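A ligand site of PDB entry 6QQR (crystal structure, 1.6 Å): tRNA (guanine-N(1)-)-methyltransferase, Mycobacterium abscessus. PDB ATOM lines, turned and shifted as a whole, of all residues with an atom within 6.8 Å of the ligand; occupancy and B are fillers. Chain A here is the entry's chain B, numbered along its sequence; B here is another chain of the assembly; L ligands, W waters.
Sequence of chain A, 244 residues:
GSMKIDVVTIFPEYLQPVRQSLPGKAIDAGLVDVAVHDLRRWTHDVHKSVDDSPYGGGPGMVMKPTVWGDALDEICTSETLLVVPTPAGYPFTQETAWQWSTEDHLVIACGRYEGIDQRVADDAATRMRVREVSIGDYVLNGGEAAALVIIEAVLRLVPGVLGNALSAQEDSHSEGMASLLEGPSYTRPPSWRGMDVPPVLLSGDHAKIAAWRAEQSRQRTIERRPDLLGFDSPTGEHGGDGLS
An oxygen (O1) of the ligand is in hydrogen-bond range of the backbone NH of Leu 140 (3.0 Å). The backbone carbonyl oxygen (O) of Tyr 138 sits at hydrogen-bond distance from an oxygen (O1) of the ligand (3.0 Å). The backbone carbonyl oxygen of Gly 111 lies within hydrogen-bond range of a nitrogen (N1) of the ligand (3.4 Å).
The side-chain hydroxyl (OH) of Tyr 138 sits at hydrogen-bond distance from the backbone carbonyl oxygen (O) of Ile 135 (3.3 Å). The backbone carbonyl oxygen (O) of Gly 111 sits at hydrogen-bond distance from the backbone NH (N) of Gly 143 (2.9 Å). The backbone NH of Thr 86 is in hydrogen-bond range of the backbone carbonyl oxygen of Val 133, at 2.9 Å. OG1 of Thr 86 sits close to N of Ala 88 (3.1 Å). The backbone NH of Asn 141 sits at hydrogen-bond distance from the side-chain carboxylate of Glu 152 of chain B (2.6 Å). N of Gly 142 lies within hydrogen-bond range of OE2 of Glu 152 of chain B (3.4 Å). The side-chain carboxylate of Glu 144 is in salt-bridge range of the guanidinium group of Arg 112 (2.9 Å).
Merely in contact with the ligand: Pro 85 (3.2 Å), Tyr 113 (3.4 Å), Val 139 (3.4 Å), Pro 87 (3.5 Å), Thr 86 (3.6 Å), Gly 143 (3.6 Å), Asn 141 (3.6 Å), Gly 142 (3.7 Å) and Arg 112 (3.8 Å). Hydrophobic or aromatic side chains that line the ligand: Pro 87 and Leu 140. Of the 26 residues printed, 12 come within 4 Å of the ligand. The nearest printed residue that does not touch the ligand is Gly 115 (4.2 Å).
Water W3 lies within hydrogen-bond range of O2 of the ligand (2.7 Å), O of Gly 136 (2.7 Å), OG of Ser 134 (2.8 Å) and O of Tyr 138 (3.2 Å). Water W2 lies within hydrogen-bond range of O2 of the ligand (2.8 Å), N of Ile 135 (3.0 Å) and O of Val 133 (3.0 Å).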
ATOM      1  N   VAL A  84     -28.600  33.442  -5.699  1.00  0.00           N
ATOM      2  CA  VAL A  84     -28.319  32.362  -4.749  1.00  0.00           C
ATOM      3  C   VAL A  84     -27.526  31.270  -5.433  1.00  0.00           C
ATOM      4  O   VAL A  84     -28.100  30.463  -6.172  1.00  0.00           O
ATOM      5  CB  VAL A  84     -29.607  31.750  -4.149  1.00  0.00           C
ATOM      6  CG1 VAL A  84     -29.245  30.758  -3.069  1.00  0.00           C
ATOM      7  CG2 VAL A  84     -30.509  32.844  -3.604  1.00  0.00           C
ATOM      8  N   PRO A  85     -26.203  31.247  -5.239  1.00  0.00           N
ATOM      9  CA  PRO A  85     -25.465  30.156  -5.874  1.00  0.00           C
ATOM     10  C   PRO A  85     -25.863  28.814  -5.280  1.00  0.00           C
ATOM     11  O   PRO A  85     -26.051  28.678  -4.073  1.00  0.00           O
ATOM     12  CB  PRO A  85     -24.006  30.482  -5.544  1.00  0.00           C
ATOM     13  CG  PRO A  85     -23.992  31.973  -5.323  1.00  0.00           C
ATOM     14  CD  PRO A  85     -25.325  32.251  -4.630  1.00  0.00           C
ATOM     15  N   THR A  86     -26.018  27.814  -6.151  1.00  0.00           N
ATOM     16  CA  THR A  86     -26.360  26.452  -5.729  1.00  0.00           C
ATOM     17  C   THR A  86     -26.065  25.505  -6.868  1.00  0.00           C
ATOM     18  O   THR A  86     -26.260  25.868  -8.016  1.00  0.00           O
ATOM     19  CB  THR A  86     -27.866  26.348  -5.293  1.00  0.00           C
ATOM     20  OG1 THR A  86     -28.246  24.967  -5.229  1.00  0.00           O
ATOM     21  CG2 THR A  86     -28.792  27.052  -6.284  1.00  0.00           C
ATOM     22  N   PRO A  87     -25.583  24.282  -6.552  1.00  0.00           N
ATOM     23  CA  PRO A  87     -25.316  23.321  -7.621  1.00  0.00           C
ATOM     24  C   PRO A  87     -26.605  22.889  -8.315  1.00  0.00           C
ATOM     25  O   PRO A  87     -26.567  22.350  -9.434  1.00  0.00           O
ATOM     26  CB  PRO A  87     -24.668  22.139  -6.882  1.00  0.00           C
ATOM     27  CG  PRO A  87     -25.095  22.293  -5.472  1.00  0.00           C
ATOM     28  CD  PRO A  87     -25.243  23.756  -5.216  1.00  0.00           C
ATOM     29  N   ALA A  88     -27.738  23.162  -7.670  1.00  0.00           N
ATOM     30  CA  ALA A  88     -29.040  22.833  -8.243  1.00  0.00           C
ATOM     31  C   ALA A  88     -29.675  24.003  -8.985  1.00  0.00           C
ATOM     32  O   ALA A  88     -30.849  23.945  -9.320  1.00  0.00           O
ATOM     33  CB  ALA A  88     -29.975  22.353  -7.136  1.00  0.00           C
ATOM     34  N   ALA A 109     -26.421  35.617  -1.881  1.00  0.00           N
ATOM     35  CA  ALA A 109     -26.586  34.881  -0.640  1.00  0.00           C
ATOM     36  C   ALA A 109     -25.789  33.604  -0.711  1.00  0.00           C
ATOM     37  O   ALA A 109     -26.138  32.678  -1.464  1.00  0.00           O
ATOM     38  CB  ALA A 109     -28.076  34.587  -0.388  1.00  0.00           C
ATOM     39  N   CYS A 110     -24.698  33.554   0.064  1.00  0.00           N
ATOM     40  CA  CYS A 110     -23.793  32.417   0.043  1.00  0.00           C
ATOM     41  C   CYS A 110     -24.135  31.406   1.118  1.00  0.00           C
ATOM     42  O   CYS A 110     -24.021  31.710   2.305  1.00  0.00           O
ATOM     43  CB  CYS A 110     -22.339  32.851   0.228  1.00  0.00           C
ATOM     44  SG  CYS A 110     -21.732  33.980  -1.035  1.00  0.00           S
ATOM     45  N   GLY A 111     -24.510  30.219   0.687  1.00  0.00           N
ATOM     46  CA  GLY A 111     -24.795  29.142   1.613  1.00  0.00           C
ATOM     47  C   GLY A 111     -23.599  28.265   1.880  1.00  0.00           C
ATOM     48  O   GLY A 111     -22.562  28.318   1.194  1.00  0.00           O
ATOM     49  N   ARG A 112     -23.735  27.460   2.922  1.00  0.00           N
ATOM     50  CA  ARG A 112     -22.745  26.481   3.347  1.00  0.00           C
ATOM     51  C   ARG A 112     -23.519  25.230   3.746  1.00  0.00           C
ATOM     52  O   ARG A 112     -24.739  25.183   3.546  1.00  0.00           O
ATOM     53  CB  ARG A 112     -21.891  27.014   4.510  1.00  0.00           C
ATOM     54  CG  ARG A 112     -20.758  27.955   4.054  1.00  0.00           C
ATOM     55  CD  ARG A 112     -19.504  27.163   3.750  1.00  0.00           C
ATOM     56  NE  ARG A 112     -18.638  27.879   2.812  1.00  0.00           N
ATOM     57  CZ  ARG A 112     -17.397  27.511   2.510  1.00  0.00           C
ATOM     58  NH1 ARG A 112     -16.868  26.442   3.102  1.00  0.00           N
ATOM     59  NH2 ARG A 112     -16.695  28.227   1.642  1.00  0.00           N
ATOM     60  N   TYR A 113     -22.830  24.239   4.291  1.00  0.00           N
ATOM     61  CA  TYR A 113     -23.458  22.966   4.663  1.00  0.00           C
ATOM     62  C   TYR A 113     -24.193  22.386   3.459  1.00  0.00           C
ATOM     63  O   TYR A 113     -23.687  22.424   2.346  1.00  0.00           O
ATOM     64  CB  TYR A 113     -24.403  23.157   5.851  1.00  0.00           C
ATOM     65  CG  TYR A 113     -23.808  23.991   6.975  1.00  0.00           C
ATOM     66  CD1 TYR A 113     -22.955  23.425   7.912  1.00  0.00           C
ATOM     67  CD2 TYR A 113     -24.110  25.343   7.106  1.00  0.00           C
ATOM     68  CE1 TYR A 113     -22.411  24.181   8.943  1.00  0.00           C
ATOM     69  CE2 TYR A 113     -23.571  26.104   8.114  1.00  0.00           C
ATOM     70  CZ  TYR A 113     -22.724  25.525   9.041  1.00  0.00           C
ATOM     71  OH  TYR A 113     -22.198  26.287  10.056  1.00  0.00           O
ATOM     72  N   GLU A 114     -25.397  21.845   3.671  1.00  0.00           N
ATOM     73  CA  GLU A 114     -26.184  21.280   2.577  1.00  0.00           C
ATOM     74  C   GLU A 114     -27.096  22.306   1.918  1.00  0.00           C
ATOM     75  O   GLU A 114     -28.019  21.950   1.183  1.00  0.00           O
ATOM     76  CB  GLU A 114     -26.997  20.083   3.070  1.00  0.00           C
ATOM     77  CG  GLU A 114     -26.162  18.992   3.691  1.00  0.00           C
ATOM     78  CD  GLU A 114     -24.954  18.637   2.832  1.00  0.00           C
ATOM     79  OE1 GLU A 114     -23.824  18.638   3.359  1.00  0.00           O
ATOM     80  OE2 GLU A 114     -25.148  18.346   1.628  1.00  0.00           O
ATOM     81  N   GLY A 115     -26.840  23.578   2.175  1.00  0.00           N
ATOM     82  CA  GLY A 115     -27.598  24.630   1.512  1.00  0.00           C
ATOM     83  C   GLY A 115     -28.561  25.343   2.440  1.00  0.00           C
ATOM     84  O   GLY A 115     -28.534  25.144   3.650  1.00  0.00           O
ATOM     85  N   ILE A 116     -29.426  26.160   1.845  1.00  0.00           N
ATOM     86  CA  ILE A 116     -30.325  27.043   2.580  1.00  0.00           C
ATOM     87  C   ILE A 116     -31.760  26.527   2.474  1.00  0.00           C
ATOM     88  O   ILE A 116     -32.182  26.143   1.388  1.00  0.00           O
ATOM     89  CB  ILE A 116     -30.266  28.482   2.015  1.00  0.00           C
ATOM     90  CG1 ILE A 116     -28.820  29.009   2.037  1.00  0.00           C
ATOM     91  CG2 ILE A 116     -31.213  29.426   2.754  1.00  0.00           C
ATOM     92  CD1 ILE A 116     -28.646  30.303   1.251  1.00  0.00           C
ATOM     93  N   VAL A 133     -28.622  29.925  -9.076  1.00  0.00           N
ATOM     94  CA  VAL A 133     -27.755  29.717 -10.240  1.00  0.00           C
ATOM     95  C   VAL A 133     -26.583  28.814  -9.909  1.00  0.00           C
ATOM     96  O   VAL A 133     -26.015  28.867  -8.808  1.00  0.00           O
ATOM     97  CB  VAL A 133     -27.186  31.042 -10.802  1.00  0.00           C
ATOM     98  CG1 VAL A 133     -28.303  31.862 -11.470  1.00  0.00           C
ATOM     99  CG2 VAL A 133     -26.473  31.839  -9.678  1.00  0.00           C
ATOM    100  N   SER A 134     -26.238  27.981 -10.891  1.00  0.00           N
ATOM    101  CA  SER A 134     -25.053  27.125 -10.824  1.00  0.00           C
ATOM    102  C   SER A 134     -23.969  27.634 -11.757  1.00  0.00           C
ATOM    103  O   SER A 134     -24.225  27.808 -12.951  1.00  0.00           O
ATOM    104  CB  SER A 134     -25.397  25.687 -11.195  1.00  0.00           C
ATOM    105  OG  SER A 134     -24.208  24.923 -11.299  1.00  0.00           O
ATOM    106  N   ILE A 135     -22.766  27.843 -11.237  1.00  0.00           N
ATOM    107  CA  ILE A 135     -21.697  28.356 -12.111  1.00  0.00           C
ATOM    108  C   ILE A 135     -21.042  27.264 -12.941  1.00  0.00           C
ATOM    109  O   ILE A 135     -20.282  27.566 -13.863  1.00  0.00           O
ATOM    110  CB  ILE A 135     -20.610  29.112 -11.329  1.00  0.00           C
ATOM    111  CG1 ILE A 135     -19.973  28.255 -10.245  1.00  0.00           C
ATOM    112  CG2 ILE A 135     -21.180  30.423 -10.752  1.00  0.00           C
ATOM    113  CD1 ILE A 135     -18.575  28.773  -9.840  1.00  0.00           C
ATOM    114  N   GLY A 136     -21.323  26.000 -12.631  1.00  0.00           N
ATOM    115  CA  GLY A 136     -20.763  24.896 -13.411  1.00  0.00           C
ATOM    116  C   GLY A 136     -21.092  23.559 -12.809  1.00  0.00           C
ATOM    117  O   GLY A 136     -21.623  23.487 -11.705  1.00  0.00           O
ATOM    118  N   TYR A 138     -20.069  21.111 -10.973  1.00  0.00           N
ATOM    119  CA  TYR A 138     -19.180  20.625  -9.927  1.00  0.00           C
ATOM    120  C   TYR A 138     -19.725  21.114  -8.600  1.00  0.00           C
ATOM    121  O   TYR A 138     -20.490  22.092  -8.532  1.00  0.00           O
ATOM    122  CB  TYR A 138     -17.739  21.092 -10.139  1.00  0.00           C
ATOM    123  CG  TYR A 138     -17.687  22.499 -10.666  1.00  0.00           C
ATOM    124  CD1 TYR A 138     -17.879  23.603  -9.823  1.00  0.00           C
ATOM    125  CD2 TYR A 138     -17.472  22.734 -12.017  1.00  0.00           C
ATOM    126  CE1 TYR A 138     -17.882  24.880 -10.324  1.00  0.00           C
ATOM    127  CE2 TYR A 138     -17.470  24.016 -12.540  1.00  0.00           C
ATOM    128  CZ  TYR A 138     -17.663  25.093 -11.680  1.00  0.00           C
ATOM    129  OH  TYR A 138     -17.670  26.354 -12.200  1.00  0.00           O
ATOM    130  N   VAL A 139     -19.321  20.440  -7.531  1.00  0.00           N
ATOM    131  CA  VAL A 139     -19.788  20.770  -6.196  1.00  0.00           C
ATOM    132  C   VAL A 139     -18.677  21.458  -5.401  1.00  0.00           C
ATOM    133  O   VAL A 139     -17.540  20.990  -5.346  1.00  0.00           O
ATOM    134  CB  VAL A 139     -20.276  19.513  -5.456  1.00  0.00           C
ATOM    135  CG1 VAL A 139     -20.800  19.881  -4.082  1.00  0.00           C
ATOM    136  CG2 VAL A 139     -21.363  18.813  -6.262  1.00  0.00           C
ATOM    137  N   LEU A 140     -19.035  22.595  -4.807  1.00  0.00           N
ATOM    138  CA  LEU A 140     -18.168  23.325  -3.890  1.00  0.00           C
ATOM    139  C   LEU A 140     -18.635  23.082  -2.449  1.00  0.00           C
ATOM    140  O   LEU A 140     -19.667  22.450  -2.219  1.00  0.00           O
ATOM    141  CB  LEU A 140     -18.186  24.809  -4.221  1.00  0.00           C
ATOM    142  CG  LEU A 140     -17.810  25.140  -5.667  1.00  0.00           C
ATOM    143  CD1 LEU A 140     -17.986  26.611  -5.944  1.00  0.00           C
ATOM    144  CD2 LEU A 140     -16.377  24.689  -5.958  1.00  0.00           C
ATOM    145  N   ASN A 141     -17.884  23.577  -1.466  1.00  0.00           N
ATOM    146  CA  ASN A 141     -18.338  23.445  -0.079  1.00  0.00           C
ATOM    147  C   ASN A 141     -19.294  24.567   0.304  1.00  0.00           C
ATOM    148  O   ASN A 141     -19.985  24.475   1.313  1.00  0.00           O
ATOM    149  CB  ASN A 141     -17.157  23.437   0.892  1.00  0.00           C
ATOM    150  CG  ASN A 141     -16.547  22.058   1.059  1.00  0.00           C
ATOM    151  OD1 ASN A 141     -17.182  21.029   0.804  1.00  0.00           O
ATOM    152  ND2 ASN A 141     -15.288  22.023   1.504  1.00  0.00           N
ATOM    153  N   GLY A 142     -19.321  25.624  -0.493  1.00  0.00           N
ATOM    154  CA  GLY A 142     -20.161  26.777  -0.212  1.00  0.00           C
ATOM    155  C   GLY A 142     -20.251  27.714  -1.393  1.00  0.00           C
ATOM    156  O   GLY A 142     -19.555  27.531  -2.388  1.00  0.00           O
ATOM    157  N   GLY A 143     -21.096  28.733  -1.273  1.00  0.00           N
ATOM    158  CA  GLY A 143     -21.343  29.654  -2.367  1.00  0.00           C
ATOM    159  C   GLY A 143     -20.308  30.743  -2.589  1.00  0.00           C
ATOM    160  O   GLY A 143     -20.383  31.459  -3.584  1.00  0.00           O
ATOM    161  N   GLU A 144     -19.344  30.876  -1.682  1.00  0.00           N
ATOM    162  CA  GLU A 144     -18.405  31.998  -1.714  1.00  0.00           C
ATOM    163  C   GLU A 144     -17.556  32.050  -2.989  1.00  0.00           C
ATOM    164  O   GLU A 144     -17.418  33.121  -3.592  1.00  0.00           O
ATOM    165  CB  GLU A 144     -17.497  31.963  -0.484  1.00  0.00           C
ATOM    166  CG  GLU A 144     -18.210  32.364   0.806  1.00  0.00           C
ATOM    167  CD  GLU A 144     -19.044  31.258   1.421  1.00  0.00           C
ATOM    168  OE1 GLU A 144     -18.932  30.090   0.987  1.00  0.00           O
ATOM    169  OE2 GLU A 144     -19.783  31.553   2.376  1.00  0.00           O
ATOM    170  N   ALA A 146     -18.256  30.759  -5.827  1.00  0.00           N
ATOM    171  CA  ALA A 146     -19.192  31.052  -6.893  1.00  0.00           C
ATOM    172  C   ALA A 146     -19.536  32.545  -6.935  1.00  0.00           C
ATOM    173  O   ALA A 146     -19.656  33.133  -8.020  1.00  0.00           O
ATOM    174  CB  ALA A 146     -20.474  30.215  -6.739  1.00  0.00           C
ATOM    175  N   GLU B 152     -11.000  24.258  -4.575  1.00  0.00           N
ATOM    176  CA  GLU B 152     -12.050  23.860  -3.659  1.00  0.00           C
ATOM    177  C   GLU B 152     -12.741  22.572  -4.113  1.00  0.00           C
ATOM    178  O   GLU B 152     -12.971  21.662  -3.308  1.00  0.00           O
ATOM    179  CB  GLU B 152     -13.082  24.965  -3.496  1.00  0.00           C
ATOM    180  CG  GLU B 152     -14.075  24.619  -2.384  1.00  0.00           C
ATOM    181  CD  GLU B 152     -15.012  25.762  -2.043  1.00  0.00           C
ATOM    182  OE1 GLU B 152     -14.660  26.927  -2.308  1.00  0.00           O
ATOM    183  OE2 GLU B 152     -16.095  25.479  -1.485  1.00  0.00           O
HETATM  184  O1  LIG L   1     -21.294  23.865  -6.254  1.00  0.00           O
HETATM  185  B1  LIG L   1     -21.663  25.210  -5.980  1.00  0.00           B
HETATM  186  O2  LIG L   1     -22.208  25.977  -7.026  1.00  0.00           O
HETATM  187  C1  LIG L   1     -22.306  25.474  -4.509  1.00  0.00           C
HETATM  188  C2  LIG L   1     -22.139  24.528  -3.496  1.00  0.00           C
HETATM  189  C3  LIG L   1     -22.735  24.773  -2.231  1.00  0.00           C
HETATM  190  C4  LIG L   1     -23.462  25.922  -2.022  1.00  0.00           C
HETATM  191  C5  LIG L   1     -23.640  26.878  -3.074  1.00  0.00           C
HETATM  192  C6  LIG L   1     -23.057  26.645  -4.292  1.00  0.00           C
HETATM  193  N1  LIG L   1     -23.936  25.921  -0.727  1.00  0.00           N
HETATM  194  C7  LIG L   1     -23.531  24.828  -0.091  1.00  0.00           C
HETATM  195  C8  LIG L   1     -22.780  24.065  -0.983  1.00  0.00           C
HETATM  196  O   HOH W   1     -26.541  27.508  -0.663  1.00  0.00           O
HETATM  197  O   HOH W   2     -23.108  28.333  -8.345  1.00  0.00           O
HETATM  198  O   HOH W   3     -22.180  24.661  -9.339  1.00  0.00           O
